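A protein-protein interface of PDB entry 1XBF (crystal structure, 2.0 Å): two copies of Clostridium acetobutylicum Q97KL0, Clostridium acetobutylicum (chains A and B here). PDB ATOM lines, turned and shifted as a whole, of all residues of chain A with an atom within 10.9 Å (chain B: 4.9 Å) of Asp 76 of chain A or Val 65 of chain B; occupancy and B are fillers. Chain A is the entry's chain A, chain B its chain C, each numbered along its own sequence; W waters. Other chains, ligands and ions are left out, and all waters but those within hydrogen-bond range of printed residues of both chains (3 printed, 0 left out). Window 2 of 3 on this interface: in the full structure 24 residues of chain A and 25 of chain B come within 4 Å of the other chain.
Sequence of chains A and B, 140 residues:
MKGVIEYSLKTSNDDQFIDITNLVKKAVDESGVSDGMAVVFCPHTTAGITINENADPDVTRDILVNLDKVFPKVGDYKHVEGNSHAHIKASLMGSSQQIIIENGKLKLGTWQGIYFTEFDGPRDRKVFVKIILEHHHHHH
Asp 76 of chain A touches just these residues of chain B: Arg 61, Asp 62, Val 65 and Asn 66.
Of the printed residues of chain B, Tyr 77 of chain A touches Asp 62 and Asn 66.
Of the printed residues of chain B, Lys 78 of chain A touches Arg 61 (3.6 Å) and Asp 62 (2.8 Å).
Of the printed residues of chain B, His 79 of chain A touches Asp 62.
Gly 82 of chain A touches none of the printed residues of chain B.
Of chain A, only Asp 76 (2.9 Å) and Lys 78 (3.6 Å) come within 4 Å of Arg 61 of chain B.
Asp 62 of chain B touches just these residues of chain A: Asp 76 (3.9 Å), Tyr 77 (3.5 Å), Lys 78 (2.8 Å), His 79 (2.9 Å) and Ser 84 (2.9 Å).
No residue of chain A comes within 4 Å of Leu 64 of chain B.
No residue of chain A comes within 4 Å of Asp 68 of chain B.
The nearest printed residue of chain B that does not touch Asp 76 of chain A is Lys 69 of chain B (6.3 Å).
The nearest printed residue of chain B that does not touch Ser 84 of chain A is Ile 63 of chain B (5.2 Å).
Water W1 bridges OH of Tyr 77 of chain A (2.7 Å) and OD1 of Asn 66 of chain B (2.7 Å).
Water W2 bridges the side-chain amide oxygen (OD1) of Asn 66 of chain B (2.8 Å) and the backbone NH (N) of Asp 76 of chain A (2.9 Å).
Water W3 lies within hydrogen-bond range of O of Val 70 of chain A (2.8 Å) and NZ of Lys 69 of chain B (2.8 Å).
The side-chain carboxylate (OD1) of Asp 76 of chain A is in salt-bridge range of the guanidinium group (NH1) of Arg 61 of chain B (3.0 Å).
ND2 of Asn 66 of chain B is in hydrogen-bond range of O of Asp 76 of chain A (3.1 Å).
OD1 of Asp 62 of chain B is in hydrogen-bond range of N of Lys 78 of chain A (2.8 Å).
The side-chain carboxylate of Asp 62 of chain B sits at hydrogen-bond distance from the backbone NH of His 79 of chain A.
The side-chain hydroxyl (OG) of Ser 84 of chain A lies within hydrogen-bond range of the side-chain carboxylate (OD2) of Asp 62 of chain B, 2.9 Å away.
Of the 17 printed residues of chain A, 7 touch a printed residue of chain B.
Hydrophobic or aromatic side chains of chain A within 4 Å of the printed part of chain B: Phe 71, Tyr 77, His 79 and Ile 88.
Of the 9 printed residues of chain B, 5 touch a printed residue of chain A.
Printed residues of chain B that touch a printed residue of chain A: Arg 61, Asp 62, Ile 63, Val 65 and Asn 66.
Hydrophobic or aromatic side chains of chain B that line the printed part of chain A: Ile 63 and Val 65.
Along chain B the printed residues that touch a printed residue of chain A span positions 61 to 66.
Among the printed residues, Asp or Glu carboxylates within 4 Å of a Lys or Arg side-chain nitrogen of the other chain: Asp 76 of chain A with Arg 61 of chain B.
OH of Tyr 77 of chain A lies within hydrogen-bond range of O of Pro 72 of chain A.
A ring nitrogen (NE2) of His 79 of chain A sits close to the side-chain carboxylate of Glu 81 of chain A, at 3.4 Å.
NH2 of Arg 61 of chain B lies within salt-bridge range of OD1 of Asp 62 of chain B (2.8 Å).
The backbone carbonyl oxygen (O) of Asp 62 of chain B sits at hydrogen-bond distance from the side-chain amide nitrogen (ND2) of Asn 66 of chain B, at 2.7 Å.
Asn 66 of chain B touches Phe 71 of chain A.
Asp 62 of chain B touches Asp 76 of chain A.
CG1 of Val 65 of chain B touches OD2 of Asp 76 of chain A, 3.7 Å away.
Asp 62 of chain B touches Tyr 77 of chain A (OD1 to CA, 3.5 Å).
Asn 66 of chain B touches Tyr 77 of chain A (ND2 to CE1, 3.5 Å).
NE of Arg 61 of chain B touches CD of Lys 78 of chain A (3.6 Å).
CG1 of Ile 88 of chain A touches CG1 of Ile 63 of chain B, 3.95 Å away.
Asn 66 of chain B touches Ile 88 of chain A (CB to CD1, 3.9 Å).
No position is printed for both chains.
Of the 13 pairs that touch across the chains among the printed residues, none has its exchanged pair printed and touching as well.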
ATOM      1  N   VAL A  70      23.558  -4.758 -30.550  1.00  0.00           N
ATOM      2  CA  VAL A  70      22.157  -4.959 -30.204  1.00  0.00           C
ATOM      3  C   VAL A  70      21.756  -6.435 -30.078  1.00  0.00           C
ATOM      4  O   VAL A  70      20.881  -6.773 -29.290  1.00  0.00           O
ATOM      5  CB  VAL A  70      21.238  -4.253 -31.248  1.00  0.00           C
ATOM      6  CG1 VAL A  70      19.767  -4.494 -30.921  1.00  0.00           C
ATOM      7  CG2 VAL A  70      21.537  -2.751 -31.265  1.00  0.00           C
ATOM      8  N   PHE A  71      22.393  -7.298 -30.863  1.00  0.00           N
ATOM      9  CA  PHE A  71      22.113  -8.736 -30.838  1.00  0.00           C
ATOM     10  C   PHE A  71      23.454  -9.452 -30.712  1.00  0.00           C
ATOM     11  O   PHE A  71      23.982  -9.984 -31.689  1.00  0.00           O
ATOM     12  CB  PHE A  71      21.409  -9.165 -32.134  1.00  0.00           C
ATOM     13  CG  PHE A  71      20.082  -8.495 -32.351  1.00  0.00           C
ATOM     14  CD1 PHE A  71      18.983  -8.825 -31.559  1.00  0.00           C
ATOM     15  CD2 PHE A  71      19.936  -7.508 -33.321  1.00  0.00           C
ATOM     16  CE1 PHE A  71      17.755  -8.175 -31.732  1.00  0.00           C
ATOM     17  CE2 PHE A  71      18.709  -6.848 -33.501  1.00  0.00           C
ATOM     18  CZ  PHE A  71      17.623  -7.185 -32.707  1.00  0.00           C
ATOM     19  N   PRO A  72      24.028  -9.470 -29.496  1.00  0.00           N
ATOM     20  CA  PRO A  72      25.319 -10.113 -29.236  1.00  0.00           C
ATOM     21  C   PRO A  72      25.357 -11.614 -29.489  1.00  0.00           C
ATOM     22  O   PRO A  72      24.318 -12.282 -29.543  1.00  0.00           O
ATOM     23  CB  PRO A  72      25.589  -9.763 -27.773  1.00  0.00           C
ATOM     24  CG  PRO A  72      24.229  -9.756 -27.189  1.00  0.00           C
ATOM     25  CD  PRO A  72      23.414  -9.010 -28.239  1.00  0.00           C
ATOM     26  N   LYS A  73      26.575 -12.126 -29.633  1.00  0.00           N
ATOM     27  CA  LYS A  73      26.816 -13.542 -29.886  1.00  0.00           C
ATOM     28  C   LYS A  73      26.378 -14.392 -28.698  1.00  0.00           C
ATOM     29  O   LYS A  73      25.905 -15.515 -28.870  1.00  0.00           O
ATOM     30  CB  LYS A  73      28.302 -13.762 -30.180  1.00  0.00           C
ATOM     31  CG  LYS A  73      28.659 -15.168 -30.626  1.00  0.00           C
ATOM     32  CD  LYS A  73      30.053 -15.207 -31.235  1.00  0.00           C
ATOM     33  CE  LYS A  73      30.357 -16.569 -31.837  1.00  0.00           C
ATOM     34  NZ  LYS A  73      31.658 -16.557 -32.561  1.00  0.00           N
ATOM     35  N   VAL A  74      26.533 -13.850 -27.493  1.00  0.00           N
ATOM     36  CA  VAL A  74      26.134 -14.562 -26.286  1.00  0.00           C
ATOM     37  C   VAL A  74      24.915 -13.899 -25.659  1.00  0.00           C
ATOM     38  O   VAL A  74      24.854 -12.673 -25.544  1.00  0.00           O
ATOM     39  CB  VAL A  74      27.283 -14.600 -25.241  1.00  0.00           C
ATOM     40  CG1 VAL A  74      28.524 -15.204 -25.865  1.00  0.00           C
ATOM     41  CG2 VAL A  74      27.579 -13.206 -24.722  1.00  0.00           C
ATOM     42  N   GLY A  75      23.945 -14.710 -25.252  1.00  0.00           N
ATOM     43  CA  GLY A  75      22.747 -14.164 -24.644  1.00  0.00           C
ATOM     44  C   GLY A  75      21.637 -15.177 -24.429  1.00  0.00           C
ATOM     45  O   GLY A  75      21.894 -16.373 -24.284  1.00  0.00           O
ATOM     46  N   ASP A  76      20.397 -14.695 -24.422  1.00  0.00           N
ATOM     47  CA  ASP A  76      19.235 -15.549 -24.198  1.00  0.00           C
ATOM     48  C   ASP A  76      18.907 -16.382 -25.434  1.00  0.00           C
ATOM     49  O   ASP A  76      17.884 -16.172 -26.089  1.00  0.00           O
ATOM     50  CB  ASP A  76      18.036 -14.683 -23.811  1.00  0.00           C
ATOM     51  CG  ASP A  76      16.879 -15.494 -23.259  1.00  0.00           C
ATOM     52  OD1 ASP A  76      17.002 -16.737 -23.166  1.00  0.00           O
ATOM     53  OD2 ASP A  76      15.844 -14.885 -22.911  1.00  0.00           O
ATOM     54  N   TYR A  77      19.773 -17.338 -25.749  1.00  0.00           N
ATOM     55  CA  TYR A  77      19.556 -18.171 -26.922  1.00  0.00           C
ATOM     56  C   TYR A  77      19.444 -19.662 -26.586  1.00  0.00           C
ATOM     57  O   TYR A  77      20.427 -20.291 -26.174  1.00  0.00           O
ATOM     58  CB  TYR A  77      20.697 -17.964 -27.925  1.00  0.00           C
ATOM     59  CG  TYR A  77      20.952 -16.516 -28.319  1.00  0.00           C
ATOM     60  CD1 TYR A  77      20.008 -15.784 -29.040  1.00  0.00           C
ATOM     61  CD2 TYR A  77      22.154 -15.890 -27.993  1.00  0.00           C
ATOM     62  CE1 TYR A  77      20.258 -14.459 -29.431  1.00  0.00           C
ATOM     63  CE2 TYR A  77      22.419 -14.573 -28.377  1.00  0.00           C
ATOM     64  CZ  TYR A  77      21.465 -13.861 -29.098  1.00  0.00           C
ATOM     65  OH  TYR A  77      21.735 -12.558 -29.483  1.00  0.00           O
ATOM     66  N   LYS A  78      18.250 -20.229 -26.768  1.00  0.00           N
ATOM     67  CA  LYS A  78      18.049 -21.652 -26.506  1.00  0.00           C
ATOM     68  C   LYS A  78      18.752 -22.467 -27.578  1.00  0.00           C
ATOM     69  O   LYS A  78      18.994 -23.660 -27.412  1.00  0.00           O
ATOM     70  CB  LYS A  78      16.560 -21.999 -26.473  1.00  0.00           C
ATOM     71  CG  LYS A  78      15.878 -21.648 -25.157  1.00  0.00           C
ATOM     72  CD  LYS A  78      14.479 -22.242 -25.078  1.00  0.00           C
ATOM     73  CE  LYS A  78      13.855 -21.983 -23.713  1.00  0.00           C
ATOM     74  NZ  LYS A  78      12.481 -22.564 -23.585  1.00  0.00           N
ATOM     75  N   HIS A  79      19.074 -21.817 -28.689  1.00  0.00           N
ATOM     76  CA  HIS A  79      19.785 -22.479 -29.772  1.00  0.00           C
ATOM     77  C   HIS A  79      21.246 -22.305 -29.381  1.00  0.00           C
ATOM     78  O   HIS A  79      21.959 -21.469 -29.929  1.00  0.00           O
ATOM     79  CB  HIS A  79      19.485 -21.777 -31.096  1.00  0.00           C
ATOM     80  CG  HIS A  79      19.950 -22.526 -32.303  1.00  0.00           C
ATOM     81  ND1 HIS A  79      20.995 -22.094 -33.090  1.00  0.00           N
ATOM     82  CD2 HIS A  79      19.496 -23.666 -32.875  1.00  0.00           C
ATOM     83  CE1 HIS A  79      21.162 -22.932 -34.096  1.00  0.00           C
ATOM     84  NE2 HIS A  79      20.263 -23.895 -33.989  1.00  0.00           N
ATOM     85  N   VAL A  80      21.672 -23.094 -28.402  1.00  0.00           N
ATOM     86  CA  VAL A  80      23.030 -23.032 -27.870  1.00  0.00           C
ATOM     87  C   VAL A  80      24.175 -23.298 -28.851  1.00  0.00           C
ATOM     88  O   VAL A  80      25.337 -23.341 -28.446  1.00  0.00           O
ATOM     89  CB  VAL A  80      23.173 -23.990 -26.665  1.00  0.00           C
ATOM     90  CG1 VAL A  80      22.262 -23.541 -25.535  1.00  0.00           C
ATOM     91  CG2 VAL A  80      22.827 -25.413 -27.085  1.00  0.00           C
ATOM     92  N   GLU A  81      23.863 -23.465 -30.134  1.00  0.00           N
ATOM     93  CA  GLU A  81      24.902 -23.716 -31.129  1.00  0.00           C
ATOM     94  C   GLU A  81      25.805 -22.498 -31.312  1.00  0.00           C
ATOM     95  O   GLU A  81      26.920 -22.609 -31.824  1.00  0.00           O
ATOM     96  CB  GLU A  81      24.270 -24.130 -32.459  1.00  0.00           C
ATOM     97  CG  GLU A  81      23.380 -25.359 -32.322  1.00  0.00           C
ATOM     98  CD  GLU A  81      22.871 -25.872 -33.653  1.00  0.00           C
ATOM     99  OE1 GLU A  81      22.043 -26.809 -33.654  1.00  0.00           O
ATOM    100  OE2 GLU A  81      23.304 -25.341 -34.698  1.00  0.00           O
ATOM    101  N   GLY A  82      25.323 -21.334 -30.887  1.00  0.00           N
ATOM    102  CA  GLY A  82      26.130 -20.132 -30.974  1.00  0.00           C
ATOM    103  C   GLY A  82      25.978 -19.204 -32.166  1.00  0.00           C
ATOM    104  O   GLY A  82      26.733 -18.238 -32.282  1.00  0.00           O
ATOM    105  N   ASN A  83      25.033 -19.475 -33.059  1.00  0.00           N
ATOM    106  CA  ASN A  83      24.851 -18.592 -34.211  1.00  0.00           C
ATOM    107  C   ASN A  83      23.403 -18.138 -34.362  1.00  0.00           C
ATOM    108  O   ASN A  83      22.946 -17.804 -35.457  1.00  0.00           O
ATOM    109  CB  ASN A  83      25.344 -19.262 -35.503  1.00  0.00           C
ATOM    110  CG  ASN A  83      24.576 -20.516 -35.846  1.00  0.00           C
ATOM    111  OD1 ASN A  83      23.687 -20.941 -35.104  1.00  0.00           O
ATOM    112  ND2 ASN A  83      24.919 -21.123 -36.981  1.00  0.00           N
ATOM    113  N   SER A  84      22.692 -18.119 -33.241  1.00  0.00           N
ATOM    114  CA  SER A  84      21.310 -17.685 -33.220  1.00  0.00           C
ATOM    115  C   SER A  84      21.302 -16.190 -33.555  1.00  0.00           C
ATOM    116  O   SER A  84      20.390 -15.690 -34.213  1.00  0.00           O
ATOM    117  CB  SER A  84      20.721 -17.926 -31.831  1.00  0.00           C
ATOM    118  OG  SER A  84      19.361 -17.558 -31.769  1.00  0.00           O
ATOM    119  N   HIS A  85      22.335 -15.481 -33.108  1.00  0.00           N
ATOM    120  CA  HIS A  85      22.434 -14.052 -33.378  1.00  0.00           C
ATOM    121  C   HIS A  85      22.544 -13.823 -34.883  1.00  0.00           C
ATOM    122  O   HIS A  85      22.073 -12.815 -35.394  1.00  0.00           O
ATOM    123  CB  HIS A  85      23.648 -13.454 -32.668  1.00  0.00           C
ATOM    124  CG  HIS A  85      24.954 -13.979 -33.166  1.00  0.00           C
ATOM    125  ND1 HIS A  85      25.255 -15.323 -33.185  1.00  0.00           N
ATOM    126  CD2 HIS A  85      26.042 -13.342 -33.656  1.00  0.00           C
ATOM    127  CE1 HIS A  85      26.473 -15.492 -33.665  1.00  0.00           C
ATOM    128  NE2 HIS A  85      26.973 -14.307 -33.958  1.00  0.00           N
ATOM    129  N   ILE A  88      19.103 -14.053 -36.491  1.00  0.00           N
ATOM    130  CA  ILE A  88      18.309 -12.848 -36.275  1.00  0.00           C
ATOM    131  C   ILE A  88      18.699 -11.776 -37.282  1.00  0.00           C
ATOM    132  O   ILE A  88      17.842 -11.201 -37.950  1.00  0.00           O
ATOM    133  CB  ILE A  88      18.514 -12.291 -34.859  1.00  0.00           C
ATOM    134  CG1 ILE A  88      17.997 -13.300 -33.832  1.00  0.00           C
ATOM    135  CG2 ILE A  88      17.788 -10.936 -34.717  1.00  0.00           C
ATOM    136  CD1 ILE A  88      18.391 -12.987 -32.380  1.00  0.00           C
ATOM    137  N   ARG B  61      12.248 -19.444 -31.737  1.00  0.00           N
ATOM    138  CA  ARG B  61      12.013 -19.003 -30.367  1.00  0.00           C
ATOM    139  C   ARG B  61      13.009 -17.888 -30.031  1.00  0.00           C
ATOM    140  O   ARG B  61      12.636 -16.881 -29.429  1.00  0.00           O
ATOM    141  CB  ARG B  61      12.178 -20.174 -29.386  1.00  0.00           C
ATOM    142  CG  ARG B  61      12.150 -19.788 -27.899  1.00  0.00           C
ATOM    143  CD  ARG B  61      13.501 -19.248 -27.438  1.00  0.00           C
ATOM    144  NE  ARG B  61      13.491 -18.872 -26.029  1.00  0.00           N
ATOM    145  CZ  ARG B  61      14.448 -18.162 -25.439  1.00  0.00           C
ATOM    146  NH1 ARG B  61      14.350 -17.861 -24.151  1.00  0.00           N
ATOM    147  NH2 ARG B  61      15.501 -17.754 -26.137  1.00  0.00           N
ATOM    148  N   ASP B  62      14.267 -18.059 -30.433  1.00  0.00           N
ATOM    149  CA  ASP B  62      15.284 -17.054 -30.143  1.00  0.00           C
ATOM    150  C   ASP B  62      15.039 -15.749 -30.882  1.00  0.00           C
ATOM    151  O   ASP B  62      15.331 -14.667 -30.366  1.00  0.00           O
ATOM    152  CB  ASP B  62      16.681 -17.572 -30.475  1.00  0.00           C
ATOM    153  CG  ASP B  62      17.119 -18.707 -29.556  1.00  0.00           C
ATOM    154  OD1 ASP B  62      16.494 -18.899 -28.495  1.00  0.00           O
ATOM    155  OD2 ASP B  62      18.091 -19.397 -29.903  1.00  0.00           O
ATOM    156  N   ILE B  63      14.512 -15.833 -32.099  1.00  0.00           N
ATOM    157  CA  ILE B  63      14.247 -14.609 -32.836  1.00  0.00           C
ATOM    158  C   ILE B  63      13.123 -13.843 -32.162  1.00  0.00           C
ATOM    159  O   ILE B  63      13.237 -12.649 -31.931  1.00  0.00           O
ATOM    160  CB  ILE B  63      13.852 -14.883 -34.300  1.00  0.00           C
ATOM    161  CG1 ILE B  63      15.005 -15.594 -35.017  1.00  0.00           C
ATOM    162  CG2 ILE B  63      13.501 -13.552 -34.998  1.00  0.00           C
ATOM    163  CD1 ILE B  63      14.657 -16.119 -36.402  1.00  0.00           C
ATOM    164  N   LEU B  64      12.041 -14.542 -31.836  1.00  0.00           N
ATOM    165  CA  LEU B  64      10.890 -13.910 -31.208  1.00  0.00           C
ATOM    166  C   LEU B  64      11.211 -13.285 -29.855  1.00  0.00           C
ATOM    167  O   LEU B  64      10.889 -12.123 -29.614  1.00  0.00           O
ATOM    168  CB  LEU B  64       9.757 -14.926 -31.047  1.00  0.00           C
ATOM    169  CG  LEU B  64       8.967 -15.245 -32.322  1.00  0.00           C
ATOM    170  CD1 LEU B  64       8.119 -16.491 -32.119  1.00  0.00           C
ATOM    171  CD2 LEU B  64       8.097 -14.058 -32.678  1.00  0.00           C
ATOM    172  N   VAL B  65      11.855 -14.051 -28.979  1.00  0.00           N
ATOM    173  CA  VAL B  65      12.181 -13.555 -27.648  1.00  0.00           C
ATOM    174  C   VAL B  65      13.178 -12.405 -27.658  1.00  0.00           C
ATOM    175  O   VAL B  65      13.009 -11.433 -26.931  1.00  0.00           O
ATOM    176  CB  VAL B  65      12.723 -14.685 -26.748  1.00  0.00           C
ATOM    177  CG1 VAL B  65      13.192 -14.112 -25.417  1.00  0.00           C
ATOM    178  CG2 VAL B  65      11.626 -15.720 -26.507  1.00  0.00           C
ATOM    179  N   ASN B  66      14.208 -12.505 -28.483  1.00  0.00           N
ATOM    180  CA  ASN B  66      15.205 -11.451 -28.542  1.00  0.00           C
ATOM    181  C   ASN B  66      14.715 -10.187 -29.240  1.00  0.00           C
ATOM    182  O   ASN B  66      15.149  -9.085 -28.915  1.00  0.00           O
ATOM    183  CB  ASN B  66      16.475 -12.001 -29.172  1.00  0.00           C
ATOM    184  CG  ASN B  66      17.249 -12.868 -28.196  1.00  0.00           C
ATOM    185  OD1 ASN B  66      18.010 -12.359 -27.368  1.00  0.00           O
ATOM    186  ND2 ASN B  66      17.021 -14.178 -28.253  1.00  0.00           N
ATOM    187  N   LEU B  67      13.798 -10.339 -30.186  1.00  0.00           N
ATOM    188  CA  LEU B  67      13.228  -9.179 -30.864  1.00  0.00           C
ATOM    189  C   LEU B  67      12.400  -8.495 -29.771  1.00  0.00           C
ATOM    190  O   LEU B  67      12.347  -7.271 -29.673  1.00  0.00           O
ATOM    191  CB  LEU B  67      12.314  -9.644 -32.004  1.00  0.00           C
ATOM    192  CG  LEU B  67      12.488  -9.127 -33.439  1.00  0.00           C
ATOM    193  CD1 LEU B  67      13.950  -8.891 -33.776  1.00  0.00           C
ATOM    194  CD2 LEU B  67      11.857 -10.152 -34.396  1.00  0.00           C
ATOM    195  N   ASP B  68      11.757  -9.315 -28.944  1.00  0.00           N
ATOM    196  CA  ASP B  68      10.935  -8.820 -27.847  1.00  0.00           C
ATOM    197  C   ASP B  68      11.792  -8.075 -26.814  1.00  0.00           C
ATOM    198  O   ASP B  68      11.378  -7.051 -26.283  1.00  0.00           O
ATOM    199  CB  ASP B  68      10.212  -9.988 -27.171  1.00  0.00           C
ATOM    200  CG  ASP B  68       9.512  -9.577 -25.882  1.00  0.00           C
ATOM    201  OD1 ASP B  68       8.529  -8.806 -25.957  1.00  0.00           O
ATOM    202  OD2 ASP B  68       9.945 -10.026 -24.795  1.00  0.00           O
ATOM    203  N   LYS B  69      12.984  -8.597 -26.543  1.00  0.00           N
ATOM    204  CA  LYS B  69      13.901  -8.005 -25.572  1.00  0.00           C
ATOM    205  C   LYS B  69      14.336  -6.605 -26.004  1.00  0.00           C
ATOM    206  O   LYS B  69      14.391  -5.678 -25.189  1.00  0.00           O
ATOM    207  CB  LYS B  69      15.137  -8.900 -25.412  1.00  0.00           C
ATOM    208  CG  LYS B  69      15.913  -8.735 -24.094  1.00  0.00           C
ATOM    209  CD  LYS B  69      16.514  -7.340 -23.904  1.00  0.00           C
ATOM    210  CE  LYS B  69      17.636  -7.030 -24.910  1.00  0.00           C
ATOM    211  NZ  LYS B  69      18.824  -7.925 -24.764  1.00  0.00           N
HETATM  212  O   HOH W   1      19.924 -10.752 -28.515  1.00  0.00           O
HETATM  213  O   HOH W   2      19.843 -11.951 -25.332  1.00  0.00           O
HETATM  214  O   HOH W   3      19.718  -8.432 -27.376  1.00  0.00           O
